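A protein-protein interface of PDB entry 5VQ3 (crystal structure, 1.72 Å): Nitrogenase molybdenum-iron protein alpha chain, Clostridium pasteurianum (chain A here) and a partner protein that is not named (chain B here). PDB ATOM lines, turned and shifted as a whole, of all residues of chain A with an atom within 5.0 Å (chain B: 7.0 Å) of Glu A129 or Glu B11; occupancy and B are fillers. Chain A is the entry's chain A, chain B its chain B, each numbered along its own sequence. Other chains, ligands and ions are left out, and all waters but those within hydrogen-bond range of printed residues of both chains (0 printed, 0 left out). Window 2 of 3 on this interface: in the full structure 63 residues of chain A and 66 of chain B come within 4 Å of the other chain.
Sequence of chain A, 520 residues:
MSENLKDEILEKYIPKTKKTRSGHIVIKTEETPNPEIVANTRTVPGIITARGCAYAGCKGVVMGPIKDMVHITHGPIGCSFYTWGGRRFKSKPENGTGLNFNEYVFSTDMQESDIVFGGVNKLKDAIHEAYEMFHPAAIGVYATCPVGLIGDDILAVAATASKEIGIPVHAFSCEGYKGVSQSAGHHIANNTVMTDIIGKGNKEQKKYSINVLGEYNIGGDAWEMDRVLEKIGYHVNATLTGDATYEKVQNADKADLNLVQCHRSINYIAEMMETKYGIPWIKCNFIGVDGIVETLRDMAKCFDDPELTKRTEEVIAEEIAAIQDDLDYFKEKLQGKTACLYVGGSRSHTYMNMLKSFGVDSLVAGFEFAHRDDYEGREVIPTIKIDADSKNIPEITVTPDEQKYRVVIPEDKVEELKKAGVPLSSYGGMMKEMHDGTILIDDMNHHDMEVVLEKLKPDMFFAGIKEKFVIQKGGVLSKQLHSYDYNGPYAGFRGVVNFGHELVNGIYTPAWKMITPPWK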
ATOM      1  N   ASP A 125       8.984 -20.872  -8.469  1.00  0.00           N
ATOM      2  CA  ASP A 125       9.904 -21.590  -9.360  1.00  0.00           C
ATOM      3  C   ASP A 125       9.369 -22.998  -9.618  1.00  0.00           C
ATOM      4  O   ASP A 125       9.452 -23.494 -10.749  1.00  0.00           O
ATOM      5  CB  ASP A 125      11.322 -21.663  -8.786  1.00  0.00           C
ATOM      6  CG  ASP A 125      12.046 -20.323  -8.839  1.00  0.00           C
ATOM      7  OD1 ASP A 125      11.605 -19.427  -9.596  1.00  0.00           O
ATOM      8  OD2 ASP A 125      13.030 -20.148  -8.100  1.00  0.00           O
ATOM      9  N   ALA A 126       8.797 -23.624  -8.580  1.00  0.00           N
ATOM     10  CA  ALA A 126       8.263 -25.000  -8.711  1.00  0.00           C
ATOM     11  C   ALA A 126       7.052 -25.016  -9.679  1.00  0.00           C
ATOM     12  O   ALA A 126       6.924 -25.901 -10.531  1.00  0.00           O
ATOM     13  CB  ALA A 126       7.890 -25.578  -7.337  1.00  0.00           C
ATOM     14  N   ILE A 127       6.166 -24.027  -9.558  1.00  0.00           N
ATOM     15  CA  ILE A 127       5.036 -23.903 -10.480  1.00  0.00           C
ATOM     16  C   ILE A 127       5.520 -23.777 -11.934  1.00  0.00           C
ATOM     17  O   ILE A 127       5.014 -24.462 -12.833  1.00  0.00           O
ATOM     18  CB  ILE A 127       4.105 -22.725 -10.137  1.00  0.00           C
ATOM     19  CG1 ILE A 127       3.478 -22.859  -8.761  1.00  0.00           C
ATOM     20  CG2 ILE A 127       3.026 -22.527 -11.205  1.00  0.00           C
ATOM     21  CD1 ILE A 127       2.919 -21.574  -8.187  1.00  0.00           C
ATOM     22  N   HIS A 128       6.491 -22.902 -12.187  1.00  0.00           N
ATOM     23  CA  HIS A 128       7.034 -22.783 -13.527  1.00  0.00           C
ATOM     24  C   HIS A 128       7.733 -24.047 -14.034  1.00  0.00           C
ATOM     25  O   HIS A 128       7.572 -24.402 -15.183  1.00  0.00           O
ATOM     26  CB  HIS A 128       7.987 -21.592 -13.611  1.00  0.00           C
ATOM     27  CG  HIS A 128       7.279 -20.279 -13.704  1.00  0.00           C
ATOM     28  ND1 HIS A 128       7.004 -19.662 -14.910  1.00  0.00           N
ATOM     29  CD2 HIS A 128       6.774 -19.474 -12.745  1.00  0.00           C
ATOM     30  CE1 HIS A 128       6.358 -18.531 -14.689  1.00  0.00           C
ATOM     31  NE2 HIS A 128       6.210 -18.390 -13.383  1.00  0.00           N
ATOM     32  N   GLU A 129       8.512 -24.715 -13.172  1.00  0.00           N
ATOM     33  CA  GLU A 129       9.138 -25.967 -13.532  1.00  0.00           C
ATOM     34  C   GLU A 129       8.096 -27.028 -13.914  1.00  0.00           C
ATOM     35  O   GLU A 129       8.280 -27.751 -14.892  1.00  0.00           O
ATOM     36  CB  GLU A 129      10.093 -26.470 -12.412  1.00  0.00           C
ATOM     37  CG  GLU A 129      11.379 -25.642 -12.352  1.00  0.00           C
ATOM     38  CD  GLU A 129      12.406 -26.084 -11.318  1.00  0.00           C
ATOM     39  OE1 GLU A 129      12.097 -26.938 -10.451  1.00  0.00           O
ATOM     40  OE2 GLU A 129      13.539 -25.558 -11.386  1.00  0.00           O
ATOM     41  N   ALA A 130       7.015 -27.124 -13.142  1.00  0.00           N
ATOM     42  CA  ALA A 130       5.959 -28.115 -13.401  1.00  0.00           C
ATOM     43  C   ALA A 130       5.265 -27.787 -14.693  1.00  0.00           C
ATOM     44  O   ALA A 130       5.055 -28.662 -15.520  1.00  0.00           O
ATOM     45  CB  ALA A 130       4.947 -28.117 -12.263  1.00  0.00           C
ATOM     46  N   TYR A 131       4.972 -26.498 -14.925  1.00  0.00           N
ATOM     47  CA  TYR A 131       4.357 -26.110 -16.179  1.00  0.00           C
ATOM     48  C   TYR A 131       5.237 -26.469 -17.386  1.00  0.00           C
ATOM     49  O   TYR A 131       4.773 -27.096 -18.322  1.00  0.00           O
ATOM     50  CB  TYR A 131       4.008 -24.631 -16.221  1.00  0.00           C
ATOM     51  CG  TYR A 131       3.560 -24.203 -17.611  1.00  0.00           C
ATOM     52  CD1 TYR A 131       2.307 -24.546 -18.081  1.00  0.00           C
ATOM     53  CD2 TYR A 131       4.413 -23.480 -18.449  1.00  0.00           C
ATOM     54  CE1 TYR A 131       1.896 -24.176 -19.359  1.00  0.00           C
ATOM     55  CE2 TYR A 131       4.020 -23.106 -19.748  1.00  0.00           C
ATOM     56  CZ  TYR A 131       2.768 -23.469 -20.196  1.00  0.00           C
ATOM     57  OH  TYR A 131       2.350 -23.139 -21.474  1.00  0.00           O
ATOM     58  N   GLU A 132       6.509 -26.108 -17.338  1.00  0.00           N
ATOM     59  CA  GLU A 132       7.425 -26.315 -18.485  1.00  0.00           C
ATOM     60  C   GLU A 132       7.677 -27.808 -18.730  1.00  0.00           C
ATOM     61  O   GLU A 132       7.725 -28.248 -19.860  1.00  0.00           O
ATOM     62  CB  GLU A 132       8.734 -25.547 -18.296  1.00  0.00           C
ATOM     63  CG  GLU A 132       8.572 -24.011 -18.326  1.00  0.00           C
ATOM     64  CD  GLU A 132       7.956 -23.442 -19.643  1.00  0.00           C
ATOM     65  OE1 GLU A 132       7.475 -22.269 -19.676  1.00  0.00           O
ATOM     66  OE2 GLU A 132       7.943 -24.151 -20.680  1.00  0.00           O
ATOM     67  N   MET A 133       7.787 -28.594 -17.661  1.00  0.00           N
ATOM     68  CA  MET A 133       8.043 -30.020 -17.825  1.00  0.00           C
ATOM     69  C   MET A 133       6.843 -30.841 -18.223  1.00  0.00           C
ATOM     70  O   MET A 133       7.006 -31.849 -18.898  1.00  0.00           O
ATOM     71  CB  MET A 133       8.626 -30.601 -16.527  1.00  0.00           C
ATOM     72  CG  MET A 133       9.991 -30.031 -16.175  1.00  0.00           C
ATOM     73  SD  MET A 133      10.592 -30.749 -14.622  1.00  0.00           S
ATOM     74  CE  MET A 133      10.384 -32.432 -15.179  1.00  0.00           C
ATOM     75  N   PHE A 134       5.650 -30.466 -17.767  1.00  0.00           N
ATOM     76  CA  PHE A 134       4.472 -31.362 -17.878  1.00  0.00           C
ATOM     77  C   PHE A 134       3.298 -30.834 -18.673  1.00  0.00           C
ATOM     78  O   PHE A 134       2.436 -31.624 -19.077  1.00  0.00           O
ATOM     79  CB  PHE A 134       3.987 -31.766 -16.467  1.00  0.00           C
ATOM     80  CG  PHE A 134       5.031 -32.484 -15.678  1.00  0.00           C
ATOM     81  CD1 PHE A 134       5.497 -33.734 -16.083  1.00  0.00           C
ATOM     82  CD2 PHE A 134       5.567 -31.916 -14.542  1.00  0.00           C
ATOM     83  CE1 PHE A 134       6.467 -34.385 -15.338  1.00  0.00           C
ATOM     84  CE2 PHE A 134       6.543 -32.553 -13.815  1.00  0.00           C
ATOM     85  CZ  PHE A 134       6.992 -33.789 -14.204  1.00  0.00           C
ATOM     86  N   ILE B   9      16.894 -34.294 -19.937  1.00  0.00           N
ATOM     87  CA  ILE B   9      16.940 -33.691 -18.614  1.00  0.00           C
ATOM     88  C   ILE B   9      17.065 -32.170 -18.613  1.00  0.00           C
ATOM     89  O   ILE B   9      17.995 -31.629 -19.184  1.00  0.00           O
ATOM     90  CB  ILE B   9      18.081 -34.282 -17.775  1.00  0.00           C
ATOM     91  CG1 ILE B   9      17.929 -35.821 -17.714  1.00  0.00           C
ATOM     92  CG2 ILE B   9      18.106 -33.640 -16.377  1.00  0.00           C
ATOM     93  CD1 ILE B   9      19.134 -36.569 -17.146  1.00  0.00           C
ATOM     94  N   VAL B  10      16.110 -31.510 -17.952  1.00  0.00           N
ATOM     95  CA  VAL B  10      16.183 -30.095 -17.650  1.00  0.00           C
ATOM     96  C   VAL B  10      16.406 -29.957 -16.130  1.00  0.00           C
ATOM     97  O   VAL B  10      15.725 -30.618 -15.330  1.00  0.00           O
ATOM     98  CB  VAL B  10      14.871 -29.378 -18.037  1.00  0.00           C
ATOM     99  CG1 VAL B  10      14.944 -27.897 -17.663  1.00  0.00           C
ATOM    100  CG2 VAL B  10      14.571 -29.582 -19.529  1.00  0.00           C
ATOM    101  N   GLU B  11      17.310 -29.052 -15.763  1.00  0.00           N
ATOM    102  CA  GLU B  11      17.632 -28.760 -14.359  1.00  0.00           C
ATOM    103  C   GLU B  11      16.400 -28.395 -13.537  1.00  0.00           C
ATOM    104  O   GLU B  11      15.631 -27.542 -13.945  1.00  0.00           O
ATOM    105  CB  GLU B  11      18.656 -27.617 -14.275  1.00  0.00           C
ATOM    106  CG  GLU B  11      20.100 -28.085 -14.091  1.00  0.00           C
ATOM    107  CD  GLU B  11      20.359 -28.693 -12.714  1.00  0.00           C
ATOM    108  OE1 GLU B  11      21.254 -28.177 -12.006  1.00  0.00           O
ATOM    109  OE2 GLU B  11      19.665 -29.674 -12.340  1.00  0.00           O
ATOM    110  N   ARG B  12      16.183 -29.128 -12.445  1.00  0.00           N
ATOM    111  CA  ARG B  12      15.134 -28.834 -11.481  1.00  0.00           C
ATOM    112  C   ARG B  12      15.801 -28.289 -10.262  1.00  0.00           C
ATOM    113  O   ARG B  12      16.578 -28.986  -9.646  1.00  0.00           O
ATOM    114  CB  ARG B  12      14.372 -30.085 -11.023  1.00  0.00           C
ATOM    115  CG  ARG B  12      13.185 -30.400 -11.865  1.00  0.00           C
ATOM    116  CD  ARG B  12      12.515 -31.704 -11.496  1.00  0.00           C
ATOM    117  NE  ARG B  12      13.431 -32.855 -11.373  1.00  0.00           N
ATOM    118  CZ  ARG B  12      13.569 -33.605 -10.284  1.00  0.00           C
ATOM    119  NH1 ARG B  12      12.878 -33.353  -9.165  1.00  0.00           N
ATOM    120  NH2 ARG B  12      14.392 -34.628 -10.303  1.00  0.00           N
ATOM    121  N   LYS B  13      15.468 -27.059  -9.901  1.00  0.00           N
ATOM    122  CA  LYS B  13      16.002 -26.441  -8.704  1.00  0.00           C
ATOM    123  C   LYS B  13      14.944 -26.277  -7.619  1.00  0.00           C
ATOM    124  O   LYS B  13      15.269 -25.974  -6.469  1.00  0.00           O
ATOM    125  CB  LYS B  13      16.591 -25.086  -9.088  1.00  0.00           C
ATOM    126  CG  LYS B  13      17.833 -25.267  -9.954  1.00  0.00           C
ATOM    127  CD  LYS B  13      18.650 -23.995 -10.138  1.00  0.00           C
ATOM    128  CE  LYS B  13      19.639 -24.140 -11.299  1.00  0.00           C
ATOM    129  NZ  LYS B  13      18.944 -24.138 -12.626  1.00  0.00           N
ATOM    130  N   ALA B  14      13.668 -26.484  -7.956  1.00  0.00           N
ATOM    131  CA  ALA B  14      12.616 -26.187  -6.985  1.00  0.00           C
ATOM    132  C   ALA B  14      11.579 -27.288  -6.823  1.00  0.00           C
ATOM    133  O   ALA B  14      11.074 -27.448  -5.745  1.00  0.00           O
ATOM    134  CB  ALA B  14      11.893 -24.902  -7.363  1.00  0.00           C
ATOM    135  N   LEU B  15      11.207 -27.937  -7.915  1.00  0.00           N
ATOM    136  CA  LEU B  15      10.147 -28.937  -7.891  1.00  0.00           C
ATOM    137  C   LEU B  15      10.783 -30.275  -7.535  1.00  0.00           C
ATOM    138  O   LEU B  15      11.536 -30.829  -8.319  1.00  0.00           O
ATOM    139  CB  LEU B  15       9.474 -29.025  -9.274  1.00  0.00           C
ATOM    140  CG  LEU B  15       8.255 -29.917  -9.393  1.00  0.00           C
ATOM    141  CD1 LEU B  15       7.109 -29.360  -8.578  1.00  0.00           C
ATOM    142  CD2 LEU B  15       7.892 -30.103 -10.855  1.00  0.00           C
ATOM    143  N   ARG B  16      10.459 -30.773  -6.347  1.00  0.00           N
ATOM    144  CA  ARG B  16      10.849 -32.095  -5.859  1.00  0.00           C
ATOM    145  C   ARG B  16       9.770 -33.112  -6.269  1.00  0.00           C
ATOM    146  O   ARG B  16       8.558 -32.866  -6.092  1.00  0.00           O
ATOM    147  CB  ARG B  16      11.006 -32.061  -4.340  1.00  0.00           C
ATOM    148  CG  ARG B  16      11.198 -33.380  -3.635  1.00  0.00           C
ATOM    149  CD  ARG B  16      12.532 -33.979  -3.961  1.00  0.00           C
ATOM    150  NE  ARG B  16      13.624 -33.121  -3.525  1.00  0.00           N
ATOM    151  CZ  ARG B  16      14.814 -33.051  -4.109  1.00  0.00           C
ATOM    152  NH1 ARG B  16      15.093 -33.785  -5.179  1.00  0.00           N
ATOM    153  NH2 ARG B  16      15.747 -32.230  -3.624  1.00  0.00           N
ATOM    154  N   LYS B 369      24.326 -38.682  -6.240  1.00  0.00           N
ATOM    155  CA  LYS B 369      23.641 -37.443  -5.873  1.00  0.00           C
ATOM    156  C   LYS B 369      23.023 -37.461  -4.480  1.00  0.00           C
ATOM    157  O   LYS B 369      22.265 -38.375  -4.122  1.00  0.00           O
ATOM    158  CB  LYS B 369      22.564 -37.095  -6.917  1.00  0.00           C
ATOM    159  CG  LYS B 369      21.902 -35.752  -6.718  1.00  0.00           C
ATOM    160  CD  LYS B 369      21.116 -35.303  -7.919  1.00  0.00           C
ATOM    161  CE  LYS B 369      20.364 -34.017  -7.642  1.00  0.00           C
ATOM    162  NZ  LYS B 369      19.560 -33.671  -8.852  1.00  0.00           N
ATOM    163  N   ASP B 376      14.958 -38.215 -10.745  1.00  0.00           N
ATOM    164  CA  ASP B 376      16.350 -38.175 -11.244  1.00  0.00           C
ATOM    165  C   ASP B 376      16.820 -39.522 -11.735  1.00  0.00           C
ATOM    166  O   ASP B 376      17.373 -39.644 -12.823  1.00  0.00           O
ATOM    167  CB  ASP B 376      17.330 -37.770 -10.141  1.00  0.00           C
ATOM    168  CG  ASP B 376      17.288 -36.280  -9.796  1.00  0.00           C
ATOM    169  OD1 ASP B 376      17.154 -35.436 -10.717  1.00  0.00           O
ATOM    170  OD2 ASP B 376      17.343 -35.985  -8.571  1.00  0.00           O
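Glu A129 touches just these residues of chain B: Glu B11 (3.9 Å), Arg B12 (3.6 Å), Lys B13 (2.9 Å), Ala B14 (3.0 Å) and Leu B15 (2.9 Å).
Glu B11 touches just one residue of chain A: Glu A129.
Of the printed residues of chain A, Lys B13 touches Glu A129.
Printed residues of chain A within 4 Å of Ala B14: Asp A125, Ala A126 and Glu A129.
Of the printed residues of chain B, Asp A125 touches Ala B14 (3.6 Å).
Of the printed residues of chain B, Ala A126 touches Ala B14 and Leu B15.
His A128 touches none of the printed residues of chain B.
The nearest printed residue of chain A that does not touch Glu B11 is Met A133 (6.0 Å).
The nearest printed residue of chain B that does not touch Asp A125 is Leu B15 (5.5 Å).
Among the printed residues, merely in contact across the chains: Asp A125 with Ala B14 (3.6 Å), Ala A126 with Ala B14 (3.6 Å), Ala A126 with Leu B15 (3.98 Å), Glu A129 with Glu B11 (3.9 Å), Glu A129 with Arg B12 (3.6 Å), Ala A130 with Leu B15 (3.8 Å) and Met A133 with Arg B12 (3.8 Å).
Hydrophobic or aromatic side chains of chain A within 4 Å of the printed part of chain B: Ala A130 and Met A133.
Along chain A the printed residues that touch a printed residue of chain B span positions 125 to 133.
Printed residues of chain B that touch a printed residue of chain A: Glu B11, Arg B12, Lys B13, Ala B14 and Leu B15.
Along chain B the printed residues that touch a printed residue of chain A span positions 11 to 15.
Among the printed residues, 10 pairs touch across the chains.
The backbone NH (N) of Lys B13 sits at hydrogen-bond distance from the side-chain carboxylate (OE2) of Glu A129 (2.9 Å).
The backbone NH (N) of Ala B14 sits at hydrogen-bond distance from the side-chain carboxylate (OE1) of Glu A129 (3.0 Å).
OE1 of Glu A129 sits at hydrogen-bond distance from N of Leu B15, 2.9 Å away.
NH1 of Arg B12 sits at hydrogen-bond distance from O of Leu B15.
The guanidinium group (NH2) of Arg B12 is in salt-bridge range of the side-chain carboxylate (OD1) of Asp B376, at 2.9 Å.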
